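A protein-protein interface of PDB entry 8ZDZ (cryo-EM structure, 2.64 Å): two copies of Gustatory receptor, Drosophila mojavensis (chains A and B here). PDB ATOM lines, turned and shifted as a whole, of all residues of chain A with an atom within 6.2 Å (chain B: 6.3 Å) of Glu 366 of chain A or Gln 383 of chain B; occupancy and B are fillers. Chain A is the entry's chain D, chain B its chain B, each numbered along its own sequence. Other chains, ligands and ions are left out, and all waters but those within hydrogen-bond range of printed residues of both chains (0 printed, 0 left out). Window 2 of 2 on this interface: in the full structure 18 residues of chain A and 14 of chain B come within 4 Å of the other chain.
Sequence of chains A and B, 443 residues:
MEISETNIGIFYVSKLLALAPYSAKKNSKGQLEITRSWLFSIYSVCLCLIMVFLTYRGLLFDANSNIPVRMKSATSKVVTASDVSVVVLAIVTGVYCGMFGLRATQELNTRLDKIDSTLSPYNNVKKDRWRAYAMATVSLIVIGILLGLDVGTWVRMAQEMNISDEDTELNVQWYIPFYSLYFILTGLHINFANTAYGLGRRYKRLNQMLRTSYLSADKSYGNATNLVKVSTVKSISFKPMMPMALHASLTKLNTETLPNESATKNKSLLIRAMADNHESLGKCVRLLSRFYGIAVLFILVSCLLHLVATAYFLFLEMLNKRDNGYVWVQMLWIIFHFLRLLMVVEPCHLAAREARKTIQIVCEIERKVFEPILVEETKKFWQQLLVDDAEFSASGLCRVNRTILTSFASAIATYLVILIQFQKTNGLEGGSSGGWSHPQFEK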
ATOM      1  N   ILE A 361     -22.942  15.988   7.361  1.00  0.00           N
ATOM      2  CA  ILE A 361     -24.157  15.379   6.825  1.00  0.00           C
ATOM      3  C   ILE A 361     -25.386  16.152   7.279  1.00  0.00           C
ATOM      4  O   ILE A 361     -26.340  16.335   6.513  1.00  0.00           O
ATOM      5  CB  ILE A 361     -24.238  13.892   7.224  1.00  0.00           C
ATOM      6  CG1 ILE A 361     -23.123  13.091   6.552  1.00  0.00           C
ATOM      7  CG2 ILE A 361     -25.593  13.309   6.872  1.00  0.00           C
ATOM      8  CD1 ILE A 361     -22.030  12.661   7.479  1.00  0.00           C
ATOM      9  N   VAL A 362     -25.382  16.627   8.524  1.00  0.00           N
ATOM     10  CA  VAL A 362     -26.519  17.395   9.023  1.00  0.00           C
ATOM     11  C   VAL A 362     -26.655  18.707   8.262  1.00  0.00           C
ATOM     12  O   VAL A 362     -27.765  19.129   7.918  1.00  0.00           O
ATOM     13  CB  VAL A 362     -26.386  17.622  10.538  1.00  0.00           C
ATOM     14  CG1 VAL A 362     -27.215  18.814  10.977  1.00  0.00           C
ATOM     15  CG2 VAL A 362     -26.821  16.379  11.278  1.00  0.00           C
ATOM     16  N   CYS A 363     -25.532  19.371   7.980  1.00  0.00           N
ATOM     17  CA  CYS A 363     -25.583  20.598   7.189  1.00  0.00           C
ATOM     18  C   CYS A 363     -26.117  20.325   5.787  1.00  0.00           C
ATOM     19  O   CYS A 363     -26.950  21.082   5.270  1.00  0.00           O
ATOM     20  CB  CYS A 363     -24.199  21.238   7.120  1.00  0.00           C
ATOM     21  SG  CYS A 363     -23.821  22.344   8.493  1.00  0.00           S
ATOM     22  N   GLU A 364     -25.651  19.244   5.160  1.00  0.00           N
ATOM     23  CA  GLU A 364     -26.135  18.899   3.826  1.00  0.00           C
ATOM     24  C   GLU A 364     -27.631  18.616   3.840  1.00  0.00           C
ATOM     25  O   GLU A 364     -28.353  18.997   2.911  1.00  0.00           O
ATOM     26  CB  GLU A 364     -25.367  17.698   3.281  1.00  0.00           C
ATOM     27  CG  GLU A 364     -23.893  17.962   3.050  1.00  0.00           C
ATOM     28  CD  GLU A 364     -23.171  16.757   2.492  1.00  0.00           C
ATOM     29  OE1 GLU A 364     -23.815  15.950   1.792  1.00  0.00           O
ATOM     30  OE2 GLU A 364     -21.959  16.614   2.757  1.00  0.00           O
ATOM     31  N   ILE A 365     -28.114  17.943   4.886  1.00  0.00           N
ATOM     32  CA  ILE A 365     -29.548  17.709   5.030  1.00  0.00           C
ATOM     33  C   ILE A 365     -30.285  19.033   5.180  1.00  0.00           C
ATOM     34  O   ILE A 365     -31.347  19.243   4.582  1.00  0.00           O
ATOM     35  CB  ILE A 365     -29.816  16.776   6.225  1.00  0.00           C
ATOM     36  CG1 ILE A 365     -29.323  15.362   5.923  1.00  0.00           C
ATOM     37  CG2 ILE A 365     -31.295  16.752   6.565  1.00  0.00           C
ATOM     38  CD1 ILE A 365     -29.044  14.548   7.165  1.00  0.00           C
ATOM     39  N   GLU A 366     -29.730  19.946   5.981  1.00  0.00           N
ATOM     40  CA  GLU A 366     -30.359  21.244   6.194  1.00  0.00           C
ATOM     41  C   GLU A 366     -30.495  22.016   4.891  1.00  0.00           C
ATOM     42  O   GLU A 366     -31.506  22.687   4.661  1.00  0.00           O
ATOM     43  CB  GLU A 366     -29.555  22.056   7.206  1.00  0.00           C
ATOM     44  CG  GLU A 366     -30.342  23.160   7.884  1.00  0.00           C
ATOM     45  CD  GLU A 366     -29.563  23.826   8.998  1.00  0.00           C
ATOM     46  OE1 GLU A 366     -28.396  23.442   9.221  1.00  0.00           O
ATOM     47  OE2 GLU A 366     -30.112  24.741   9.643  1.00  0.00           O
ATOM     48  N   ARG A 367     -29.487  21.937   4.026  1.00  0.00           N
ATOM     49  CA  ARG A 367     -29.551  22.639   2.750  1.00  0.00           C
ATOM     50  C   ARG A 367     -30.495  21.983   1.750  1.00  0.00           C
ATOM     51  O   ARG A 367     -30.628  22.491   0.632  1.00  0.00           O
ATOM     52  CB  ARG A 367     -28.160  22.750   2.131  1.00  0.00           C
ATOM     53  CG  ARG A 367     -27.460  24.064   2.414  1.00  0.00           C
ATOM     54  CD  ARG A 367     -25.979  23.940   2.143  1.00  0.00           C
ATOM     55  NE  ARG A 367     -25.733  23.153   0.942  1.00  0.00           N
ATOM     56  CZ  ARG A 367     -24.551  22.669   0.592  1.00  0.00           C
ATOM     57  NH1 ARG A 367     -23.473  22.879   1.330  1.00  0.00           N
ATOM     58  NH2 ARG A 367     -24.448  21.952  -0.523  1.00  0.00           N
ATOM     59  N   LYS A 368     -31.145  20.880   2.110  1.00  0.00           N
ATOM     60  CA  LYS A 368     -32.015  20.142   1.197  1.00  0.00           C
ATOM     61  C   LYS A 368     -33.323  19.767   1.883  1.00  0.00           C
ATOM     62  O   LYS A 368     -33.797  18.635   1.792  1.00  0.00           O
ATOM     63  CB  LYS A 368     -31.307  18.897   0.674  1.00  0.00           C
ATOM     64  CG  LYS A 368     -31.542  18.617  -0.801  1.00  0.00           C
ATOM     65  CD  LYS A 368     -30.704  17.441  -1.280  1.00  0.00           C
ATOM     66  CE  LYS A 368     -29.255  17.570  -0.837  1.00  0.00           C
ATOM     67  NZ  LYS A 368     -28.642  18.850  -1.287  1.00  0.00           N
ATOM     68  N   VAL A 369     -33.928  20.722   2.587  1.00  0.00           N
ATOM     69  CA  VAL A 369     -35.185  20.498   3.289  1.00  0.00           C
ATOM     70  C   VAL A 369     -36.098  21.695   3.073  1.00  0.00           C
ATOM     71  O   VAL A 369     -35.688  22.841   3.290  1.00  0.00           O
ATOM     72  CB  VAL A 369     -34.961  20.255   4.793  1.00  0.00           C
ATOM     73  CG1 VAL A 369     -36.230  20.555   5.563  1.00  0.00           C
ATOM     74  CG2 VAL A 369     -34.515  18.825   5.034  1.00  0.00           C
ATOM     75  N   VAL A 375     -37.098  20.915   9.494  1.00  0.00           N
ATOM     76  CA  VAL A 375     -35.882  21.723   9.428  1.00  0.00           C
ATOM     77  C   VAL A 375     -35.602  22.357  10.784  1.00  0.00           C
ATOM     78  O   VAL A 375     -34.443  22.597  11.132  1.00  0.00           O
ATOM     79  CB  VAL A 375     -35.951  22.785   8.313  1.00  0.00           C
ATOM     80  CG1 VAL A 375     -36.947  23.873   8.636  1.00  0.00           C
ATOM     81  CG2 VAL A 375     -34.573  23.379   8.053  1.00  0.00           C
ATOM     82  N   THR A 378     -33.827  19.697  12.488  1.00  0.00           N
ATOM     83  CA  THR A 378     -32.470  19.624  11.958  1.00  0.00           C
ATOM     84  C   THR A 378     -31.593  20.732  12.526  1.00  0.00           C
ATOM     85  O   THR A 378     -30.406  20.517  12.792  1.00  0.00           O
ATOM     86  CB  THR A 378     -32.499  19.693  10.434  1.00  0.00           C
ATOM     87  OG1 THR A 378     -33.570  18.878   9.942  1.00  0.00           O
ATOM     88  CG2 THR A 378     -31.188  19.192   9.859  1.00  0.00           C
ATOM     89  N   LYS A 379     -32.155  21.928  12.702  1.00  0.00           N
ATOM     90  CA  LYS A 379     -31.409  23.011  13.334  1.00  0.00           C
ATOM     91  C   LYS A 379     -31.061  22.664  14.774  1.00  0.00           C
ATOM     92  O   LYS A 379     -29.957  22.958  15.243  1.00  0.00           O
ATOM     93  CB  LYS A 379     -32.212  24.310  13.278  1.00  0.00           C
ATOM     94  CG  LYS A 379     -32.364  24.888  11.882  1.00  0.00           C
ATOM     95  CD  LYS A 379     -32.332  26.408  11.902  1.00  0.00           C
ATOM     96  CE  LYS A 379     -33.213  26.970  13.005  1.00  0.00           C
ATOM     97  NZ  LYS A 379     -34.573  27.311  12.513  1.00  0.00           N
ATOM     98  N   TRP A 382     -28.183  20.283  14.606  1.00  0.00           N
ATOM     99  CA  TRP A 382     -26.941  20.985  14.304  1.00  0.00           C
ATOM    100  C   TRP A 382     -26.421  21.729  15.526  1.00  0.00           C
ATOM    101  O   TRP A 382     -25.215  21.734  15.796  1.00  0.00           O
ATOM    102  CB  TRP A 382     -27.152  21.950  13.139  1.00  0.00           C
ATOM    103  CG  TRP A 382     -25.923  22.720  12.773  1.00  0.00           C
ATOM    104  CD1 TRP A 382     -24.970  22.359  11.869  1.00  0.00           C
ATOM    105  CD2 TRP A 382     -25.513  23.985  13.302  1.00  0.00           C
ATOM    106  NE1 TRP A 382     -23.992  23.319  11.803  1.00  0.00           N
ATOM    107  CE2 TRP A 382     -24.304  24.329  12.674  1.00  0.00           C
ATOM    108  CE3 TRP A 382     -26.055  24.860  14.248  1.00  0.00           C
ATOM    109  CZ2 TRP A 382     -23.624  25.508  12.960  1.00  0.00           C
ATOM    110  CZ3 TRP A 382     -25.378  26.030  14.531  1.00  0.00           C
ATOM    111  CH2 TRP A 382     -24.176  26.344  13.889  1.00  0.00           C
ATOM    112  N   ILE B 359     -15.396  32.937   5.688  1.00  0.00           N
ATOM    113  CA  ILE B 359     -16.406  33.250   6.690  1.00  0.00           C
ATOM    114  C   ILE B 359     -16.441  34.749   6.979  1.00  0.00           C
ATOM    115  O   ILE B 359     -17.512  35.311   7.233  1.00  0.00           O
ATOM    116  CB  ILE B 359     -16.171  32.411   7.960  1.00  0.00           C
ATOM    117  CG1 ILE B 359     -17.390  32.482   8.875  1.00  0.00           C
ATOM    118  CG2 ILE B 359     -14.910  32.846   8.687  1.00  0.00           C
ATOM    119  CD1 ILE B 359     -17.769  31.155   9.480  1.00  0.00           C
ATOM    120  N   THR B 378     -27.665  33.431   3.074  1.00  0.00           N
ATOM    121  CA  THR B 378     -26.375  33.826   3.631  1.00  0.00           C
ATOM    122  C   THR B 378     -26.189  33.277   5.039  1.00  0.00           C
ATOM    123  O   THR B 378     -25.080  32.885   5.418  1.00  0.00           O
ATOM    124  CB  THR B 378     -26.247  35.346   3.628  1.00  0.00           C
ATOM    125  OG1 THR B 378     -26.748  35.863   2.389  1.00  0.00           O
ATOM    126  CG2 THR B 378     -24.794  35.751   3.785  1.00  0.00           C
ATOM    127  N   LYS B 379     -27.259  33.259   5.836  1.00  0.00           N
ATOM    128  CA  LYS B 379     -27.186  32.656   7.162  1.00  0.00           C
ATOM    129  C   LYS B 379     -26.896  31.166   7.067  1.00  0.00           C
ATOM    130  O   LYS B 379     -26.121  30.623   7.862  1.00  0.00           O
ATOM    131  CB  LYS B 379     -28.486  32.900   7.926  1.00  0.00           C
ATOM    132  CG  LYS B 379     -28.716  34.348   8.318  1.00  0.00           C
ATOM    133  CD  LYS B 379     -29.395  34.459   9.673  1.00  0.00           C
ATOM    134  CE  LYS B 379     -30.564  33.493   9.791  1.00  0.00           C
ATOM    135  NZ  LYS B 379     -31.856  34.139   9.435  1.00  0.00           N
ATOM    136  N   LYS B 380     -27.517  30.485   6.101  1.00  0.00           N
ATOM    137  CA  LYS B 380     -27.214  29.070   5.893  1.00  0.00           C
ATOM    138  C   LYS B 380     -25.750  28.876   5.506  1.00  0.00           C
ATOM    139  O   LYS B 380     -25.091  27.944   5.984  1.00  0.00           O
ATOM    140  CB  LYS B 380     -28.133  28.485   4.822  1.00  0.00           C
ATOM    141  CG  LYS B 380     -29.415  27.885   5.367  1.00  0.00           C
ATOM    142  CD  LYS B 380     -29.963  26.824   4.429  1.00  0.00           C
ATOM    143  CE  LYS B 380     -31.388  26.443   4.792  1.00  0.00           C
ATOM    144  NZ  LYS B 380     -32.280  26.442   3.601  1.00  0.00           N
ATOM    145  N   PHE B 381     -25.232  29.747   4.641  1.00  0.00           N
ATOM    146  CA  PHE B 381     -23.824  29.680   4.261  1.00  0.00           C
ATOM    147  C   PHE B 381     -22.918  29.884   5.469  1.00  0.00           C
ATOM    148  O   PHE B 381     -21.923  29.170   5.638  1.00  0.00           O
ATOM    149  CB  PHE B 381     -23.533  30.728   3.185  1.00  0.00           C
ATOM    150  CG  PHE B 381     -22.253  30.497   2.429  1.00  0.00           C
ATOM    151  CD1 PHE B 381     -21.507  29.348   2.619  1.00  0.00           C
ATOM    152  CD2 PHE B 381     -21.799  31.438   1.524  1.00  0.00           C
ATOM    153  CE1 PHE B 381     -20.335  29.147   1.925  1.00  0.00           C
ATOM    154  CE2 PHE B 381     -20.628  31.241   0.827  1.00  0.00           C
ATOM    155  CZ  PHE B 381     -19.895  30.093   1.028  1.00  0.00           C
ATOM    156  N   TRP B 382     -23.245  30.858   6.318  1.00  0.00           N
ATOM    157  CA  TRP B 382     -22.443  31.104   7.512  1.00  0.00           C
ATOM    158  C   TRP B 382     -22.483  29.908   8.452  1.00  0.00           C
ATOM    159  O   TRP B 382     -21.460  29.531   9.034  1.00  0.00           O
ATOM    160  CB  TRP B 382     -22.934  32.364   8.225  1.00  0.00           C
ATOM    161  CG  TRP B 382     -22.168  32.680   9.470  1.00  0.00           C
ATOM    162  CD1 TRP B 382     -21.054  33.458   9.570  1.00  0.00           C
ATOM    163  CD2 TRP B 382     -22.462  32.227  10.796  1.00  0.00           C
ATOM    164  NE1 TRP B 382     -20.633  33.515  10.876  1.00  0.00           N
ATOM    165  CE2 TRP B 382     -21.482  32.767  11.648  1.00  0.00           C
ATOM    166  CE3 TRP B 382     -23.457  31.416  11.344  1.00  0.00           C
ATOM    167  CZ2 TRP B 382     -21.468  32.524  13.017  1.00  0.00           C
ATOM    168  CZ3 TRP B 382     -23.442  31.173  12.703  1.00  0.00           C
ATOM    169  CH2 TRP B 382     -22.454  31.726  13.524  1.00  0.00           C
ATOM    170  N   GLN B 383     -23.661  29.302   8.617  1.00  0.00           N
ATOM    171  CA  GLN B 383     -23.776  28.121   9.463  1.00  0.00           C
ATOM    172  C   GLN B 383     -22.935  26.975   8.919  1.00  0.00           C
ATOM    173  O   GLN B 383     -22.274  26.262   9.683  1.00  0.00           O
ATOM    174  CB  GLN B 383     -25.240  27.702   9.575  1.00  0.00           C
ATOM    175  CG  GLN B 383     -25.791  27.739  10.985  1.00  0.00           C
ATOM    176  CD  GLN B 383     -27.267  27.410  11.032  1.00  0.00           C
ATOM    177  OE1 GLN B 383     -28.097  28.268  11.331  1.00  0.00           O
ATOM    178  NE2 GLN B 383     -27.604  26.162  10.732  1.00  0.00           N
ATOM    179  N   GLN B 384     -22.950  26.783   7.599  1.00  0.00           N
ATOM    180  CA  GLN B 384     -22.136  25.730   6.999  1.00  0.00           C
ATOM    181  C   GLN B 384     -20.650  26.005   7.187  1.00  0.00           C
ATOM    182  O   GLN B 384     -19.872  25.086   7.467  1.00  0.00           O
ATOM    183  CB  GLN B 384     -22.478  25.590   5.516  1.00  0.00           C
ATOM    184  CG  GLN B 384     -21.365  25.002   4.673  1.00  0.00           C
ATOM    185  CD  GLN B 384     -21.693  25.017   3.198  1.00  0.00           C
ATOM    186  OE1 GLN B 384     -22.859  24.976   2.810  1.00  0.00           O
ATOM    187  NE2 GLN B 384     -20.663  25.079   2.363  1.00  0.00           N
ATOM    188  N   LEU B 385     -20.237  27.263   7.037  1.00  0.00           N
ATOM    189  CA  LEU B 385     -18.820  27.593   7.155  1.00  0.00           C
ATOM    190  C   LEU B 385     -18.328  27.512   8.592  1.00  0.00           C
ATOM    191  O   LEU B 385     -17.151  27.218   8.821  1.00  0.00           O
ATOM    192  CB  LEU B 385     -18.551  28.986   6.594  1.00  0.00           C
ATOM    193  CG  LEU B 385     -18.659  29.124   5.081  1.00  0.00           C
ATOM    194  CD1 LEU B 385     -18.680  30.584   4.702  1.00  0.00           C
ATOM    195  CD2 LEU B 385     -17.511  28.410   4.407  1.00  0.00           C
ATOM    196  N   LEU B 386     -19.200  27.783   9.566  1.00  0.00           N
ATOM    197  CA  LEU B 386     -18.772  27.757  10.961  1.00  0.00           C
ATOM    198  C   LEU B 386     -18.276  26.373  11.359  1.00  0.00           C
ATOM    199  O   LEU B 386     -17.231  26.241  12.007  1.00  0.00           O
ATOM    200  CB  LEU B 386     -19.918  28.198  11.870  1.00  0.00           C
ATOM    201  CG  LEU B 386     -19.745  27.966  13.369  1.00  0.00           C
ATOM    202  CD1 LEU B 386     -18.517  28.688  13.889  1.00  0.00           C
ATOM    203  CD2 LEU B 386     -20.982  28.421  14.119  1.00  0.00           C
ATOM    204  N   VAL B 387     -19.007  25.333  10.976  1.00  0.00           N
ATOM    205  CA  VAL B 387     -18.591  23.951  11.204  1.00  0.00           C
ATOM    206  C   VAL B 387     -18.010  23.439   9.885  1.00  0.00           C
ATOM    207  O   VAL B 387     -18.707  22.971   8.982  1.00  0.00           O
ATOM    208  CB  VAL B 387     -19.726  23.100  11.784  1.00  0.00           C
ATOM    209  CG1 VAL B 387     -20.423  23.882  12.871  1.00  0.00           C
ATOM    210  CG2 VAL B 387     -20.804  22.764  10.764  1.00  0.00           C
ATOM    211  N   ASP B 388     -16.695  23.571   9.754  1.00  0.00           N
ATOM    212  CA  ASP B 388     -16.005  23.207   8.525  1.00  0.00           C
ATOM    213  C   ASP B 388     -14.510  23.237   8.784  1.00  0.00           C
ATOM    214  O   ASP B 388     -14.026  24.094   9.525  1.00  0.00           O
ATOM    215  CB  ASP B 388     -16.362  24.164   7.378  1.00  0.00           C
ATOM    216  CG  ASP B 388     -15.485  23.969   6.158  1.00  0.00           C
ATOM    217  OD1 ASP B 388     -14.400  24.582   6.096  1.00  0.00           O
ATOM    218  OD2 ASP B 388     -15.882  23.202   5.255  1.00  0.00           O
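The side-chain carboxylate (OE2) of Glu 366 of chain A sits at hydrogen-bond distance from the side-chain amide nitrogen (NE2) of Gln 383 of chain B. The side-chain amide oxygen (OE1) of Gln 384 of chain B lies within hydrogen-bond range of the guanidinium group (NH1) of Arg 367 of chain A, 2.6 Å away.
The side-chain sulfur (SG) of Cys 363 of chain A is in hydrogen-bond range of the indole nitrogen (NE1) of Trp 382 of chain A, at 3.5 Å.
SG of Cys 363 of chain A touches CG2 of Val 387 of chain B (3.8 Å). O of Glu 366 of chain A touches CE of Lys 380 of chain B (3.8 Å). Trp 382 of chain A touches Gln 383 of chain B (CH2 to CG, 3.6 Å). Trp 382 of chain A touches Leu 386 of chain B (CH2 to CD2, 3.8 Å). Trp 382 of chain A touches Val 387 of chain B (NE1 to CG2, 3.4 Å).
Of the printed residues of chain B, Cys 363 of chain A touches Val 387 (3.8 Å). Glu 364 of chain A touches none of the printed residues of chain B. Of chain B, only Lys 380 (3.8 Å) and Gln 383 (3.1 Å) come within 4 Å of Glu 366 of chain A. Printed residues of chain B within 4 Å of Arg 367 of chain A: Gln 384 (2.6 Å). Of the printed residues of chain A, Lys 380 of chain B touches Glu 366. Printed residues of chain A within 4 Å of Gln 383 of chain B: Glu 366 (3.1 Å) and Trp 382 (3.6 Å). Printed residues of chain A within 4 Å of Gln 384 of chain B: Arg 367. Printed residues of chain A within 4 Å of Leu 386 of chain B: Trp 382 (3.8 Å). The nearest printed residue of chain B that does not touch Glu 366 of chain A is Gln 384 of chain B (6.6 Å). The nearest residue of chain A that does not touch Gln 383 of chain B is Cys 363 of chain A (4.4 Å).
Hydrophobic or aromatic side chains of chain B that line the printed part of chain A: Leu 386 and Val 387. Printed residues of chain A that touch a printed residue of chain B: Cys 363, Glu 366, Arg 367 and Trp 382. Hydrophobic or aromatic side chains of chain A within 4 Å of the printed part of chain B: Trp 382.
Positions printed for both chains: 378, 379 and 382. Of the 7 pairs that touch across the chains among the printed residues, none has its exchanged pair printed and touching as well.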
